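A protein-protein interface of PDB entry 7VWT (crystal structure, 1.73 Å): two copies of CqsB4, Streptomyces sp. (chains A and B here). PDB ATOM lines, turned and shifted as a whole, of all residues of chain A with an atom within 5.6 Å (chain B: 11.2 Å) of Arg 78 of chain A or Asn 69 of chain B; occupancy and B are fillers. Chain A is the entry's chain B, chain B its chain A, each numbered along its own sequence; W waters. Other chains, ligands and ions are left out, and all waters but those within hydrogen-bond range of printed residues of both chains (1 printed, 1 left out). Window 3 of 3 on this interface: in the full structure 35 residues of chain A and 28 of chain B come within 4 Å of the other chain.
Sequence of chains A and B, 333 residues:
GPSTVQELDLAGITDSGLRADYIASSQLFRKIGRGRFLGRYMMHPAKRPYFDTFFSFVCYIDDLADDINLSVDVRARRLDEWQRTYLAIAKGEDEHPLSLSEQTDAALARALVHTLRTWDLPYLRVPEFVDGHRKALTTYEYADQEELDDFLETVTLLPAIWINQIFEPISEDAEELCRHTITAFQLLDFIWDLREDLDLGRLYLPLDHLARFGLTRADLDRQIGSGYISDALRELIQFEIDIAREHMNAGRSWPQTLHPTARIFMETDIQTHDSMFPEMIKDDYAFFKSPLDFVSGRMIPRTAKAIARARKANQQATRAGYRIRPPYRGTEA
Of the 16 printed residues of chain A, 6 touch a printed residue of chain B.
Printed residues of chain A that touch a printed residue of chain B: Tyr 60, Asp 63, Leu 64, Asp 67, Leu 70 and Arg 78.
Among the printed residues, 7 pairs touch across the chains.
Asp 67 of chain B touches its own counterpart, Asp 67 of chain A.
Leu 70 of chain A touches its own counterpart, Leu 70 of chain B.
Positions printed for both chains: 63, 64, 67, 70, 73, 74, 75, 76 and 78.
Of the 7 pairs that touch across the chains among the printed residues, 2 have their exchanged pair printed and touching as well.
The backbone carbonyl oxygen (O) of Asn 69 of chain B sits at hydrogen-bond distance from the guanidinium group (NH1) of Arg 78 of chain A (2.7 Å).
OD2 of Asp 67 of chain B sits close to OD2 of Asp 67 of chain A.
The side-chain amide nitrogen (ND2) of Asn 69 of chain B sits at hydrogen-bond distance from the side-chain carboxylate (OD2) of Asp 67 of chain A, at 3.0 Å.
Water W1 lies within hydrogen-bond range of OD1 of Asn 69 of chain B, O of Tyr 60 of chain A and N of Leu 64 of chain A.
CE2 of Tyr 60 of chain A touches OD1 of Asn 69 of chain B (3.7 Å).
Asp 63 of chain A touches Asn 69 of chain B.
Leu 64 of chain A touches Asn 69 of chain B.
Leu 70 of chain B touches Leu 70 of chain A.
Arg 78 of chain A touches one residue of chain B.
Asn 69 of chain B touches just these residues of chain A: Tyr 60, Asp 63, Leu 64, Asp 67 and Arg 78.
Leu 64 of chain A touches just one residue of chain B: Asn 69 (3.7 Å).
No residue of chain B comes within 4 Å of Ala 76 of chain A.
No residue of chain B comes within 4 Å of Arg 77 of chain A.
No residue of chain B comes within 4 Å of Leu 79 of chain A.
Of the printed residues of chain A, Leu 70 of chain B touches Leu 70.
Of the printed residues of chain A, Asp 67 of chain B touches Asp 67.
Of the printed residues of chain B, Tyr 60 of chain A touches Asn 69 (3.7 Å).
Printed residues of chain B within 4 Å of Leu 70 of chain A: Leu 70.
Ala 76 of chain B touches none of the printed residues of chain A.
The nearest residue of chain B that does not touch Arg 78 of chain A is Leu 70 of chain B (4.9 Å).
The nearest residue of chain A that does not touch Asn 69 of chain B is Leu 70 of chain A (4.1 Å).
The guanidinium group of Arg 75 of chain B sits at hydrogen-bond distance from the backbone carbonyl oxygen of Leu 70 of chain B, 3.0 Å away.
O of Asp 67 of chain A lies within hydrogen-bond range of NE of Arg 75 of chain A (3.0 Å).
O of Asp 67 of chain B lies within hydrogen-bond range of NE of Arg 75 of chain B.
OD1 of Asp 67 of chain B lies within hydrogen-bond range of N of Asn 69 of chain B (2.9 Å).
The backbone carbonyl oxygen (O) of Leu 70 of chain A is in hydrogen-bond range of the guanidinium group (NE) of Arg 75 of chain A (2.9 Å).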
ATOM      1  N   TYR A  60     -19.165  32.454  -4.491  1.00  0.00           N
ATOM      2  CA  TYR A  60     -19.196  31.331  -5.416  1.00  0.00           C
ATOM      3  C   TYR A  60     -19.396  30.026  -4.672  1.00  0.00           C
ATOM      4  O   TYR A  60     -20.248  29.215  -5.045  1.00  0.00           O
ATOM      5  CB  TYR A  60     -17.901  31.279  -6.244  1.00  0.00           C
ATOM      6  CG  TYR A  60     -17.864  30.026  -7.091  1.00  0.00           C
ATOM      7  CD1 TYR A  60     -17.092  28.932  -6.708  1.00  0.00           C
ATOM      8  CD2 TYR A  60     -18.629  29.920  -8.244  1.00  0.00           C
ATOM      9  CE1 TYR A  60     -17.071  27.773  -7.457  1.00  0.00           C
ATOM     10  CE2 TYR A  60     -18.618  28.757  -8.997  1.00  0.00           C
ATOM     11  CZ  TYR A  60     -17.832  27.694  -8.602  1.00  0.00           C
ATOM     12  OH  TYR A  60     -17.818  26.533  -9.343  1.00  0.00           O
ATOM     13  N   ASP A  63     -22.946  29.847  -3.130  1.00  0.00           N
ATOM     14  CA  ASP A  63     -23.956  29.553  -4.152  1.00  0.00           C
ATOM     15  C   ASP A  63     -23.884  28.111  -4.632  1.00  0.00           C
ATOM     16  O   ASP A  63     -24.914  27.465  -4.853  1.00  0.00           O
ATOM     17  CB  ASP A  63     -23.790  30.491  -5.357  1.00  0.00           C
ATOM     18  CG  ASP A  63     -24.255  31.901  -5.060  1.00  0.00           C
ATOM     19  OD1 ASP A  63     -24.728  32.160  -3.918  1.00  0.00           O
ATOM     20  OD2 ASP A  63     -24.123  32.755  -5.964  1.00  0.00           O
ATOM     21  N   LEU A  64     -22.679  27.587  -4.810  1.00  0.00           N
ATOM     22  CA  LEU A  64     -22.558  26.205  -5.246  1.00  0.00           C
ATOM     23  C   LEU A  64     -23.148  25.265  -4.206  1.00  0.00           C
ATOM     24  O   LEU A  64     -23.904  24.347  -4.534  1.00  0.00           O
ATOM     25  CB  LEU A  64     -21.091  25.870  -5.505  1.00  0.00           C
ATOM     26  CG  LEU A  64     -20.842  24.403  -5.819  1.00  0.00           C
ATOM     27  CD1 LEU A  64     -21.640  23.969  -7.005  1.00  0.00           C
ATOM     28  CD2 LEU A  64     -19.333  24.170  -6.061  1.00  0.00           C
ATOM     29  N   ASP A  67     -27.111  25.461  -4.332  1.00  0.00           N
ATOM     30  CA  ASP A  67     -27.838  25.342  -5.604  1.00  0.00           C
ATOM     31  C   ASP A  67     -28.683  24.057  -5.645  1.00  0.00           C
ATOM     32  O   ASP A  67     -28.172  22.944  -5.889  1.00  0.00           O
ATOM     33  CB  ASP A  67     -26.827  25.387  -6.746  1.00  0.00           C
ATOM     34  CG  ASP A  67     -27.459  25.677  -8.084  1.00  0.00           C
ATOM     35  OD1 ASP A  67     -28.659  25.383  -8.265  1.00  0.00           O
ATOM     36  OD2 ASP A  67     -26.723  26.196  -8.952  1.00  0.00           O
ATOM     37  N   LEU A  70     -28.806  21.066  -8.240  1.00  0.00           N
ATOM     38  CA  LEU A  70     -27.921  19.914  -8.151  1.00  0.00           C
ATOM     39  C   LEU A  70     -28.277  19.124  -6.910  1.00  0.00           C
ATOM     40  O   LEU A  70     -28.696  19.704  -5.907  1.00  0.00           O
ATOM     41  CB  LEU A  70     -26.446  20.344  -8.058  1.00  0.00           C
ATOM     42  CG  LEU A  70     -25.922  21.183  -9.214  1.00  0.00           C
ATOM     43  CD1 LEU A  70     -24.605  21.859  -8.838  1.00  0.00           C
ATOM     44  CD2 LEU A  70     -25.801  20.329 -10.476  1.00  0.00           C
ATOM     45  N   ASP A  73     -25.529  15.197  -3.216  1.00  0.00           N
ATOM     46  CA  ASP A  73     -24.344  14.382  -3.500  1.00  0.00           C
ATOM     47  C   ASP A  73     -23.498  15.008  -4.606  1.00  0.00           C
ATOM     48  O   ASP A  73     -22.266  14.980  -4.548  1.00  0.00           O
ATOM     49  CB  ASP A  73     -24.732  12.948  -3.875  1.00  0.00           C
ATOM     50  CG  ASP A  73     -24.942  12.058  -2.661  1.00  0.00           C
ATOM     51  OD1 ASP A  73     -24.691  12.519  -1.524  1.00  0.00           O
ATOM     52  OD2 ASP A  73     -25.363  10.890  -2.846  1.00  0.00           O
ATOM     53  N   VAL A  74     -24.132  15.597  -5.614  1.00  0.00           N
ATOM     54  CA  VAL A  74     -23.332  16.195  -6.670  1.00  0.00           C
ATOM     55  C   VAL A  74     -22.647  17.460  -6.163  1.00  0.00           C
ATOM     56  O   VAL A  74     -21.504  17.746  -6.531  1.00  0.00           O
ATOM     57  CB  VAL A  74     -24.186  16.457  -7.923  1.00  0.00           C
ATOM     58  CG1 VAL A  74     -23.474  17.471  -8.811  1.00  0.00           C
ATOM     59  CG2 VAL A  74     -24.408  15.121  -8.671  1.00  0.00           C
ATOM     60  N   ARG A  75     -23.335  18.247  -5.321  1.00  0.00           N
ATOM     61  CA  ARG A  75     -22.695  19.435  -4.744  1.00  0.00           C
ATOM     62  C   ARG A  75     -21.489  19.072  -3.882  1.00  0.00           C
ATOM     63  O   ARG A  75     -20.496  19.801  -3.883  1.00  0.00           O
ATOM     64  CB  ARG A  75     -23.698  20.247  -3.927  1.00  0.00           C
ATOM     65  CG  ARG A  75     -24.653  21.054  -4.780  1.00  0.00           C
ATOM     66  CD  ARG A  75     -25.730  21.783  -3.943  1.00  0.00           C
ATOM     67  NE  ARG A  75     -26.998  21.036  -3.899  1.00  0.00           N
ATOM     68  CZ  ARG A  75     -27.959  21.194  -2.978  1.00  0.00           C
ATOM     69  NH1 ARG A  75     -27.818  22.088  -1.986  1.00  0.00           N
ATOM     70  NH2 ARG A  75     -29.075  20.456  -3.053  1.00  0.00           N
ATOM     71  N   ALA A  76     -21.563  17.970  -3.117  1.00  0.00           N
ATOM     72  CA  ALA A  76     -20.403  17.548  -2.323  1.00  0.00           C
ATOM     73  C   ALA A  76     -19.220  17.189  -3.215  1.00  0.00           C
ATOM     74  O   ALA A  76     -18.066  17.541  -2.922  1.00  0.00           O
ATOM     75  CB  ALA A  76     -20.763  16.365  -1.427  1.00  0.00           C
ATOM     76  N   ARG A  77     -19.485  16.453  -4.291  1.00  0.00           N
ATOM     77  CA  ARG A  77     -18.441  16.145  -5.260  1.00  0.00           C
ATOM     78  C   ARG A  77     -17.868  17.422  -5.859  1.00  0.00           C
ATOM     79  O   ARG A  77     -16.650  17.601  -5.934  1.00  0.00           O
ATOM     80  CB  ARG A  77     -19.004  15.238  -6.363  1.00  0.00           C
ATOM     81  CG  ARG A  77     -17.978  14.403  -7.117  1.00  0.00           C
ATOM     82  CD  ARG A  77     -18.580  13.789  -8.399  1.00  0.00           C
ATOM     83  NE  ARG A  77     -18.801  14.819  -9.419  1.00  0.00           N
ATOM     84  CZ  ARG A  77     -19.981  15.130  -9.952  1.00  0.00           C
ATOM     85  NH1 ARG A  77     -21.071  14.465  -9.589  1.00  0.00           N
ATOM     86  NH2 ARG A  77     -20.068  16.100 -10.862  1.00  0.00           N
ATOM     87  N   ARG A  78     -18.741  18.324  -6.314  1.00  0.00           N
ATOM     88  CA  ARG A  78     -18.260  19.543  -6.936  1.00  0.00           C
ATOM     89  C   ARG A  78     -17.483  20.415  -5.954  1.00  0.00           C
ATOM     90  O   ARG A  78     -16.505  21.056  -6.338  1.00  0.00           O
ATOM     91  CB  ARG A  78     -19.440  20.312  -7.524  1.00  0.00           C
ATOM     92  CG  ARG A  78     -20.062  19.565  -8.690  1.00  0.00           C
ATOM     93  CD  ARG A  78     -19.264  19.812  -9.980  1.00  0.00           C
ATOM     94  NE  ARG A  78     -19.013  21.242 -10.178  1.00  0.00           N
ATOM     95  CZ  ARG A  78     -19.906  22.088 -10.708  1.00  0.00           C
ATOM     96  NH1 ARG A  78     -21.095  21.643 -11.101  1.00  0.00           N
ATOM     97  NH2 ARG A  78     -19.617  23.372 -10.853  1.00  0.00           N
ATOM     98  N   LEU A  79     -17.928  20.500  -4.700  1.00  0.00           N
ATOM     99  CA  LEU A  79     -17.135  21.203  -3.696  1.00  0.00           C
ATOM    100  C   LEU A  79     -15.780  20.534  -3.534  1.00  0.00           C
ATOM    101  O   LEU A  79     -14.737  21.196  -3.496  1.00  0.00           O
ATOM    102  CB  LEU A  79     -17.872  21.240  -2.358  1.00  0.00           C
ATOM    103  CG  LEU A  79     -19.115  22.131  -2.404  1.00  0.00           C
ATOM    104  CD1 LEU A  79     -19.952  21.987  -1.145  1.00  0.00           C
ATOM    105  CD2 LEU A  79     -18.718  23.598  -2.643  1.00  0.00           C
ATOM    106  N   ASP A  80     -15.784  19.211  -3.460  1.00  0.00           N
ATOM    107  CA  ASP A  80     -14.536  18.487  -3.273  1.00  0.00           C
ATOM    108  C   ASP A  80     -13.599  18.713  -4.455  1.00  0.00           C
ATOM    109  O   ASP A  80     -12.392  18.910  -4.269  1.00  0.00           O
ATOM    110  CB  ASP A  80     -14.853  17.006  -3.039  1.00  0.00           C
ATOM    111  CG  ASP A  80     -13.636  16.190  -2.657  1.00  0.00           C
ATOM    112  OD1 ASP A  80     -13.106  15.481  -3.530  1.00  0.00           O
ATOM    113  OD2 ASP A  80     -13.194  16.274  -1.494  1.00  0.00           O
ATOM    114  N   GLU A  81     -14.140  18.710  -5.679  1.00  0.00           N
ATOM    115  CA  GLU A  81     -13.329  18.976  -6.867  1.00  0.00           C
ATOM    116  C   GLU A  81     -12.764  20.396  -6.858  1.00  0.00           C
ATOM    117  O   GLU A  81     -11.615  20.618  -7.240  1.00  0.00           O
ATOM    118  CB  GLU A  81     -14.157  18.746  -8.135  1.00  0.00           C
ATOM    119  CG  GLU A  81     -14.455  17.272  -8.442  1.00  0.00           C
ATOM    120  CD  GLU A  81     -15.681  17.080  -9.343  1.00  0.00           C
ATOM    121  OE1 GLU A  81     -16.168  15.929  -9.429  1.00  0.00           O
ATOM    122  OE2 GLU A  81     -16.161  18.070  -9.953  1.00  0.00           O
ATOM    123  N   TRP A  82     -13.555  21.384  -6.444  1.00  0.00           N
ATOM    124  CA  TRP A  82     -13.007  22.733  -6.407  1.00  0.00           C
ATOM    125  C   TRP A  82     -11.877  22.835  -5.386  1.00  0.00           C
ATOM    126  O   TRP A  82     -10.873  23.508  -5.637  1.00  0.00           O
ATOM    127  CB  TRP A  82     -14.102  23.752  -6.087  1.00  0.00           C
ATOM    128  CG  TRP A  82     -13.634  25.149  -6.292  1.00  0.00           C
ATOM    129  CD1 TRP A  82     -13.835  25.923  -7.407  1.00  0.00           C
ATOM    130  CD2 TRP A  82     -12.856  25.946  -5.377  1.00  0.00           C
ATOM    131  NE1 TRP A  82     -13.264  27.175  -7.217  1.00  0.00           N
ATOM    132  CE2 TRP A  82     -12.653  27.210  -5.987  1.00  0.00           C
ATOM    133  CE3 TRP A  82     -12.351  25.730  -4.088  1.00  0.00           C
ATOM    134  CZ2 TRP A  82     -11.928  28.243  -5.363  1.00  0.00           C
ATOM    135  CZ3 TRP A  82     -11.634  26.767  -3.470  1.00  0.00           C
ATOM    136  CH2 TRP A  82     -11.445  28.008  -4.110  1.00  0.00           C
ATOM    137  N   GLN A  83     -12.069  22.212  -4.212  1.00  0.00           N
ATOM    138  CA  GLN A  83     -11.056  22.041  -3.167  1.00  0.00           C
ATOM    139  C   GLN A  83      -9.739  21.518  -3.724  1.00  0.00           C
ATOM    140  O   GLN A  83      -8.660  22.079  -3.486  1.00  0.00           O
ATOM    141  CB  GLN A  83     -11.578  21.024  -2.145  1.00  0.00           C
ATOM    142  CG  GLN A  83     -11.805  21.486  -0.758  1.00  0.00           C
ATOM    143  CD  GLN A  83     -12.285  20.326   0.115  1.00  0.00           C
ATOM    144  OE1 GLN A  83     -12.688  20.510   1.267  1.00  0.00           O
ATOM    145  NE2 GLN A  83     -12.264  19.126  -0.451  1.00  0.00           N
ATOM    146  N   LYS B  31     -36.420  36.431  -4.745  1.00  0.00           N
ATOM    147  CA  LYS B  31     -35.069  35.871  -4.667  1.00  0.00           C
ATOM    148  C   LYS B  31     -34.317  35.975  -5.987  1.00  0.00           C
ATOM    149  O   LYS B  31     -33.132  36.340  -6.002  1.00  0.00           O
ATOM    150  CB  LYS B  31     -35.177  34.403  -4.258  1.00  0.00           C
ATOM    151  CG  LYS B  31     -33.848  33.640  -4.157  1.00  0.00           C
ATOM    152  CD  LYS B  31     -34.081  32.169  -3.854  1.00  0.00           C
ATOM    153  CE  LYS B  31     -32.906  31.532  -3.109  1.00  0.00           C
ATOM    154  NZ  LYS B  31     -31.674  31.476  -3.947  1.00  0.00           N
ATOM    155  N   ASP B  62     -35.142  31.725 -17.155  1.00  0.00           N
ATOM    156  CA  ASP B  62     -33.868  32.435 -17.319  1.00  0.00           C
ATOM    157  C   ASP B  62     -32.798  31.893 -16.372  1.00  0.00           C
ATOM    158  O   ASP B  62     -31.653  31.633 -16.782  1.00  0.00           O
ATOM    159  CB  ASP B  62     -34.031  33.942 -17.069  1.00  0.00           C
ATOM    160  CG  ASP B  62     -34.453  34.716 -18.291  1.00  0.00           C
ATOM    161  OD1 ASP B  62     -35.052  35.817 -18.129  1.00  0.00           O
ATOM    162  OD2 ASP B  62     -34.171  34.257 -19.419  1.00  0.00           O
ATOM    163  N   ASP B  63     -33.154  31.756 -15.085  1.00  0.00           N
ATOM    164  CA  ASP B  63     -32.158  31.382 -14.072  1.00  0.00           C
ATOM    165  C   ASP B  63     -31.673  29.954 -14.272  1.00  0.00           C
ATOM    166  O   ASP B  63     -30.474  29.674 -14.133  1.00  0.00           O
ATOM    167  CB  ASP B  63     -32.732  31.535 -12.659  1.00  0.00           C
ATOM    168  CG  ASP B  63     -31.658  31.507 -11.570  1.00  0.00           C
ATOM    169  OD1 ASP B  63     -30.830  32.436 -11.514  1.00  0.00           O
ATOM    170  OD2 ASP B  63     -31.655  30.563 -10.747  1.00  0.00           O
ATOM    171  N   LEU B  64     -32.591  29.025 -14.564  1.00  0.00           N
ATOM    172  CA  LEU B  64     -32.179  27.673 -14.910  1.00  0.00           C
ATOM    173  C   LEU B  64     -31.256  27.693 -16.114  1.00  0.00           C
ATOM    174  O   LEU B  64     -30.231  27.014 -16.134  1.00  0.00           O
ATOM    175  CB  LEU B  64     -33.399  26.803 -15.202  1.00  0.00           C
ATOM    176  CG  LEU B  64     -34.399  26.610 -14.073  1.00  0.00           C
ATOM    177  CD1 LEU B  64     -35.531  25.780 -14.592  1.00  0.00           C
ATOM    178  CD2 LEU B  64     -33.734  25.889 -12.883  1.00  0.00           C
ATOM    179  N   ALA B  65     -31.617  28.466 -17.139  1.00  0.00           N
ATOM    180  CA  ALA B  65     -30.829  28.515 -18.362  1.00  0.00           C
ATOM    181  C   ALA B  65     -29.460  29.156 -18.147  1.00  0.00           C
ATOM    182  O   ALA B  65     -28.541  28.920 -18.941  1.00  0.00           O
ATOM    183  CB  ALA B  65     -31.609  29.273 -19.445  1.00  0.00           C
ATOM    184  N   ASP B  66     -29.301  29.956 -17.096  1.00  0.00           N
ATOM    185  CA  ASP B  66     -28.095  30.751 -16.907  1.00  0.00           C
ATOM    186  C   ASP B  66     -27.202  30.251 -15.787  1.00  0.00           C
ATOM    187  O   ASP B  66     -26.119  30.812 -15.607  1.00  0.00           O
ATOM    188  CB  ASP B  66     -28.444  32.217 -16.589  1.00  0.00           C
ATOM    189  CG  ASP B  66     -28.887  33.010 -17.801  1.00  0.00           C
ATOM    190  OD1 ASP B  66     -28.922  32.464 -18.930  1.00  0.00           O
ATOM    191  OD2 ASP B  66     -29.220  34.198 -17.610  1.00  0.00           O
ATOM    192  N   ASP B  67     -27.639  29.243 -15.016  1.00  0.00           N
ATOM    193  CA  ASP B  67     -26.962  28.805 -13.790  1.00  0.00           C
ATOM    194  C   ASP B  67     -25.534  28.332 -14.068  1.00  0.00           C
ATOM    195  O   ASP B  67     -25.326  27.269 -14.661  1.00  0.00           O
ATOM    196  CB  ASP B  67     -27.765  27.683 -13.102  1.00  0.00           C
ATOM    197  CG  ASP B  67     -27.238  27.341 -11.703  1.00  0.00           C
ATOM    198  OD1 ASP B  67     -26.083  27.733 -11.390  1.00  0.00           O
ATOM    199  OD2 ASP B  67     -27.980  26.667 -10.926  1.00  0.00           O
ATOM    200  N   ILE B  68     -24.544  29.103 -13.606  1.00  0.00           N
ATOM    201  CA  ILE B  68     -23.149  28.797 -13.929  1.00  0.00           C
ATOM    202  C   ILE B  68     -22.695  27.497 -13.299  1.00  0.00           C
ATOM    203  O   ILE B  68     -21.697  26.927 -13.744  1.00  0.00           O
ATOM    204  CB  ILE B  68     -22.209  29.945 -13.497  1.00  0.00           C
ATOM    205  CG1 ILE B  68     -22.306  30.198 -11.984  1.00  0.00           C
ATOM    206  CG2 ILE B  68     -22.528  31.224 -14.238  1.00  0.00           C
ATOM    207  CD1 ILE B  68     -21.206  31.165 -11.451  1.00  0.00           C
ATOM    208  N   ASN B  69     -23.390  26.992 -12.271  1.00  0.00           N
ATOM    209  CA  ASN B  69     -22.952  25.733 -11.663  1.00  0.00           C
ATOM    210  C   ASN B  69     -23.338  24.500 -12.472  1.00  0.00           C
ATOM    211  O   ASN B  69     -22.852  23.403 -12.164  1.00  0.00           O
ATOM    212  CB  ASN B  69     -23.526  25.603 -10.253  1.00  0.00           C
ATOM    213  CG  ASN B  69     -23.073  26.741  -9.344  1.00  0.00           C
ATOM    214  OD1 ASN B  69     -21.928  27.159  -9.404  1.00  0.00           O
ATOM    215  ND2 ASN B  69     -23.969  27.229  -8.498  1.00  0.00           N
ATOM    216  N   LEU B  70     -24.180  24.646 -13.481  1.00  0.00           N
ATOM    217  CA  LEU B  70     -24.623  23.546 -14.329  1.00  0.00           C
ATOM    218  C   LEU B  70     -24.007  23.676 -15.712  1.00  0.00           C
ATOM    219  O   LEU B  70     -23.979  24.772 -16.282  1.00  0.00           O
ATOM    220  CB  LEU B  70     -26.147  23.541 -14.488  1.00  0.00           C
ATOM    221  CG  LEU B  70     -27.109  23.167 -13.368  1.00  0.00           C
ATOM    222  CD1 LEU B  70     -26.557  23.532 -12.030  1.00  0.00           C
ATOM    223  CD2 LEU B  70     -28.431  23.951 -13.611  1.00  0.00           C
ATOM    224  N   SER B  71     -23.579  22.549 -16.266  1.00  0.00           N
ATOM    225  CA  SER B  71     -23.205  22.508 -17.671  1.00  0.00           C
ATOM    226  C   SER B  71     -24.437  22.767 -18.543  1.00  0.00           C
ATOM    227  O   SER B  71     -25.578  22.699 -18.089  1.00  0.00           O
ATOM    228  CB  SER B  71     -22.580  21.154 -18.022  1.00  0.00           C
ATOM    229  OG  SER B  71     -23.527  20.089 -17.920  1.00  0.00           O
ATOM    230  N   VAL B  72     -24.198  23.051 -19.818  1.00  0.00           N
ATOM    231  CA  VAL B  72     -25.313  23.254 -20.732  1.00  0.00           C
ATOM    232  C   VAL B  72     -26.192  22.001 -20.823  1.00  0.00           C
ATOM    233  O   VAL B  72     -27.422  22.102 -20.875  1.00  0.00           O
ATOM    234  CB  VAL B  72     -24.794  23.720 -22.105  1.00  0.00           C
ATOM    235  CG1 VAL B  72     -25.889  23.585 -23.142  1.00  0.00           C
ATOM    236  CG2 VAL B  72     -24.389  25.182 -22.002  1.00  0.00           C
ATOM    237  N   ASP B  73     -25.602  20.805 -20.782  1.00  0.00           N
ATOM    238  CA  ASP B  73     -26.440  19.611 -20.848  1.00  0.00           C
ATOM    239  C   ASP B  73     -27.312  19.468 -19.611  1.00  0.00           C
ATOM    240  O   ASP B  73     -28.437  18.963 -19.701  1.00  0.00           O
ATOM    241  CB  ASP B  73     -25.596  18.350 -21.021  1.00  0.00           C
ATOM    242  CG  ASP B  73     -24.905  18.282 -22.381  1.00  0.00           C
ATOM    243  OD1 ASP B  73     -25.091  19.175 -23.252  1.00  0.00           O
ATOM    244  OD2 ASP B  73     -24.150  17.318 -22.571  1.00  0.00           O
ATOM    245  N   VAL B  74     -26.805  19.864 -18.442  1.00  0.00           N
ATOM    246  CA  VAL B  74     -27.616  19.750 -17.231  1.00  0.00           C
ATOM    247  C   VAL B  74     -28.676  20.834 -17.197  1.00  0.00           C
ATOM    248  O   VAL B  74     -29.784  20.607 -16.672  1.00  0.00           O
ATOM    249  CB  VAL B  74     -26.741  19.770 -15.953  1.00  0.00           C
ATOM    250  CG1 VAL B  74     -27.593  19.978 -14.699  1.00  0.00           C
ATOM    251  CG2 VAL B  74     -25.958  18.495 -15.847  1.00  0.00           C
ATOM    252  N   ARG B  75     -28.375  22.012 -17.756  1.00  0.00           N
ATOM    253  CA  ARG B  75     -29.393  23.050 -17.852  1.00  0.00           C
ATOM    254  C   ARG B  75     -30.541  22.599 -18.746  1.00  0.00           C
ATOM    255  O   ARG B  75     -31.709  22.814 -18.418  1.00  0.00           O
ATOM    256  CB  ARG B  75     -28.789  24.346 -18.382  1.00  0.00           C
ATOM    257  CG  ARG B  75     -27.985  25.084 -17.333  1.00  0.00           C
ATOM    258  CD  ARG B  75     -27.421  26.350 -17.874  1.00  0.00           C
ATOM    259  NE  ARG B  75     -25.981  26.274 -17.947  1.00  0.00           N
ATOM    260  CZ  ARG B  75     -25.208  27.238 -18.432  1.00  0.00           C
ATOM    261  NH1 ARG B  75     -25.748  28.352 -18.889  1.00  0.00           N
ATOM    262  NH2 ARG B  75     -23.894  27.078 -18.455  1.00  0.00           N
ATOM    263  N   ALA B  76     -30.215  22.009 -19.903  1.00  0.00           N
ATOM    264  CA  ALA B  76     -31.240  21.487 -20.805  1.00  0.00           C
ATOM    265  C   ALA B  76     -32.080  20.427 -20.124  1.00  0.00           C
ATOM    266  O   ALA B  76     -33.303  20.384 -20.293  1.00  0.00           O
ATOM    267  CB  ALA B  76     -30.598  20.907 -22.078  1.00  0.00           C
ATOM    268  N   ARG B  78     -32.664  20.268 -16.860  1.00  0.00           N
ATOM    269  CA  ARG B  78     -33.528  20.965 -15.900  1.00  0.00           C
ATOM    270  C   ARG B  78     -34.698  21.619 -16.605  1.00  0.00           C
ATOM    271  O   ARG B  78     -35.813  21.631 -16.078  1.00  0.00           O
ATOM    272  CB  ARG B  78     -32.760  22.034 -15.082  1.00  0.00           C
ATOM    273  CG  ARG B  78     -31.985  21.485 -13.899  1.00  0.00           C
ATOM    274  CD  ARG B  78     -32.889  20.987 -12.781  1.00  0.00           C
ATOM    275  NE  ARG B  78     -33.643  22.044 -12.109  1.00  0.00           N
ATOM    276  CZ  ARG B  78     -34.982  22.084 -12.046  1.00  0.00           C
ATOM    277  NH1 ARG B  78     -35.715  21.110 -12.593  1.00  0.00           N
ATOM    278  NH2 ARG B  78     -35.589  23.055 -11.399  1.00  0.00           N
ATOM    279  N   LEU B 137     -29.547  27.605 -25.727  1.00  0.00           N
ATOM    280  CA  LEU B 137     -28.405  27.052 -24.999  1.00  0.00           C
ATOM    281  C   LEU B 137     -27.302  26.521 -25.922  1.00  0.00           C
ATOM    282  O   LEU B 137     -26.112  26.571 -25.560  1.00  0.00           O
ATOM    283  CB  LEU B 137     -28.876  25.937 -24.075  1.00  0.00           C
ATOM    284  CG  LEU B 137     -29.531  26.273 -22.733  1.00  0.00           C
ATOM    285  CD1 LEU B 137     -29.965  24.980 -22.137  1.00  0.00           C
ATOM    286  CD2 LEU B 137     -28.587  27.003 -21.781  1.00  0.00           C
ATOM    287  N   LEU B 200     -18.729  33.577 -22.815  1.00  0.00           N
ATOM    288  CA  LEU B 200     -19.502  32.344 -22.766  1.00  0.00           C
ATOM    289  C   LEU B 200     -19.559  31.647 -24.116  1.00  0.00           C
ATOM    290  O   LEU B 200     -20.183  30.584 -24.227  1.00  0.00           O
ATOM    291  CB  LEU B 200     -20.918  32.642 -22.257  1.00  0.00           C
ATOM    292  CG  LEU B 200     -20.919  33.017 -20.784  1.00  0.00           C
ATOM    293  CD1 LEU B 200     -22.307  33.322 -20.233  1.00  0.00           C
ATOM    294  CD2 LEU B 200     -20.249  31.880 -20.005  1.00  0.00           C
HETATM  295  O   HOH W   1     -21.683  29.273  -7.599  1.00  0.00           O
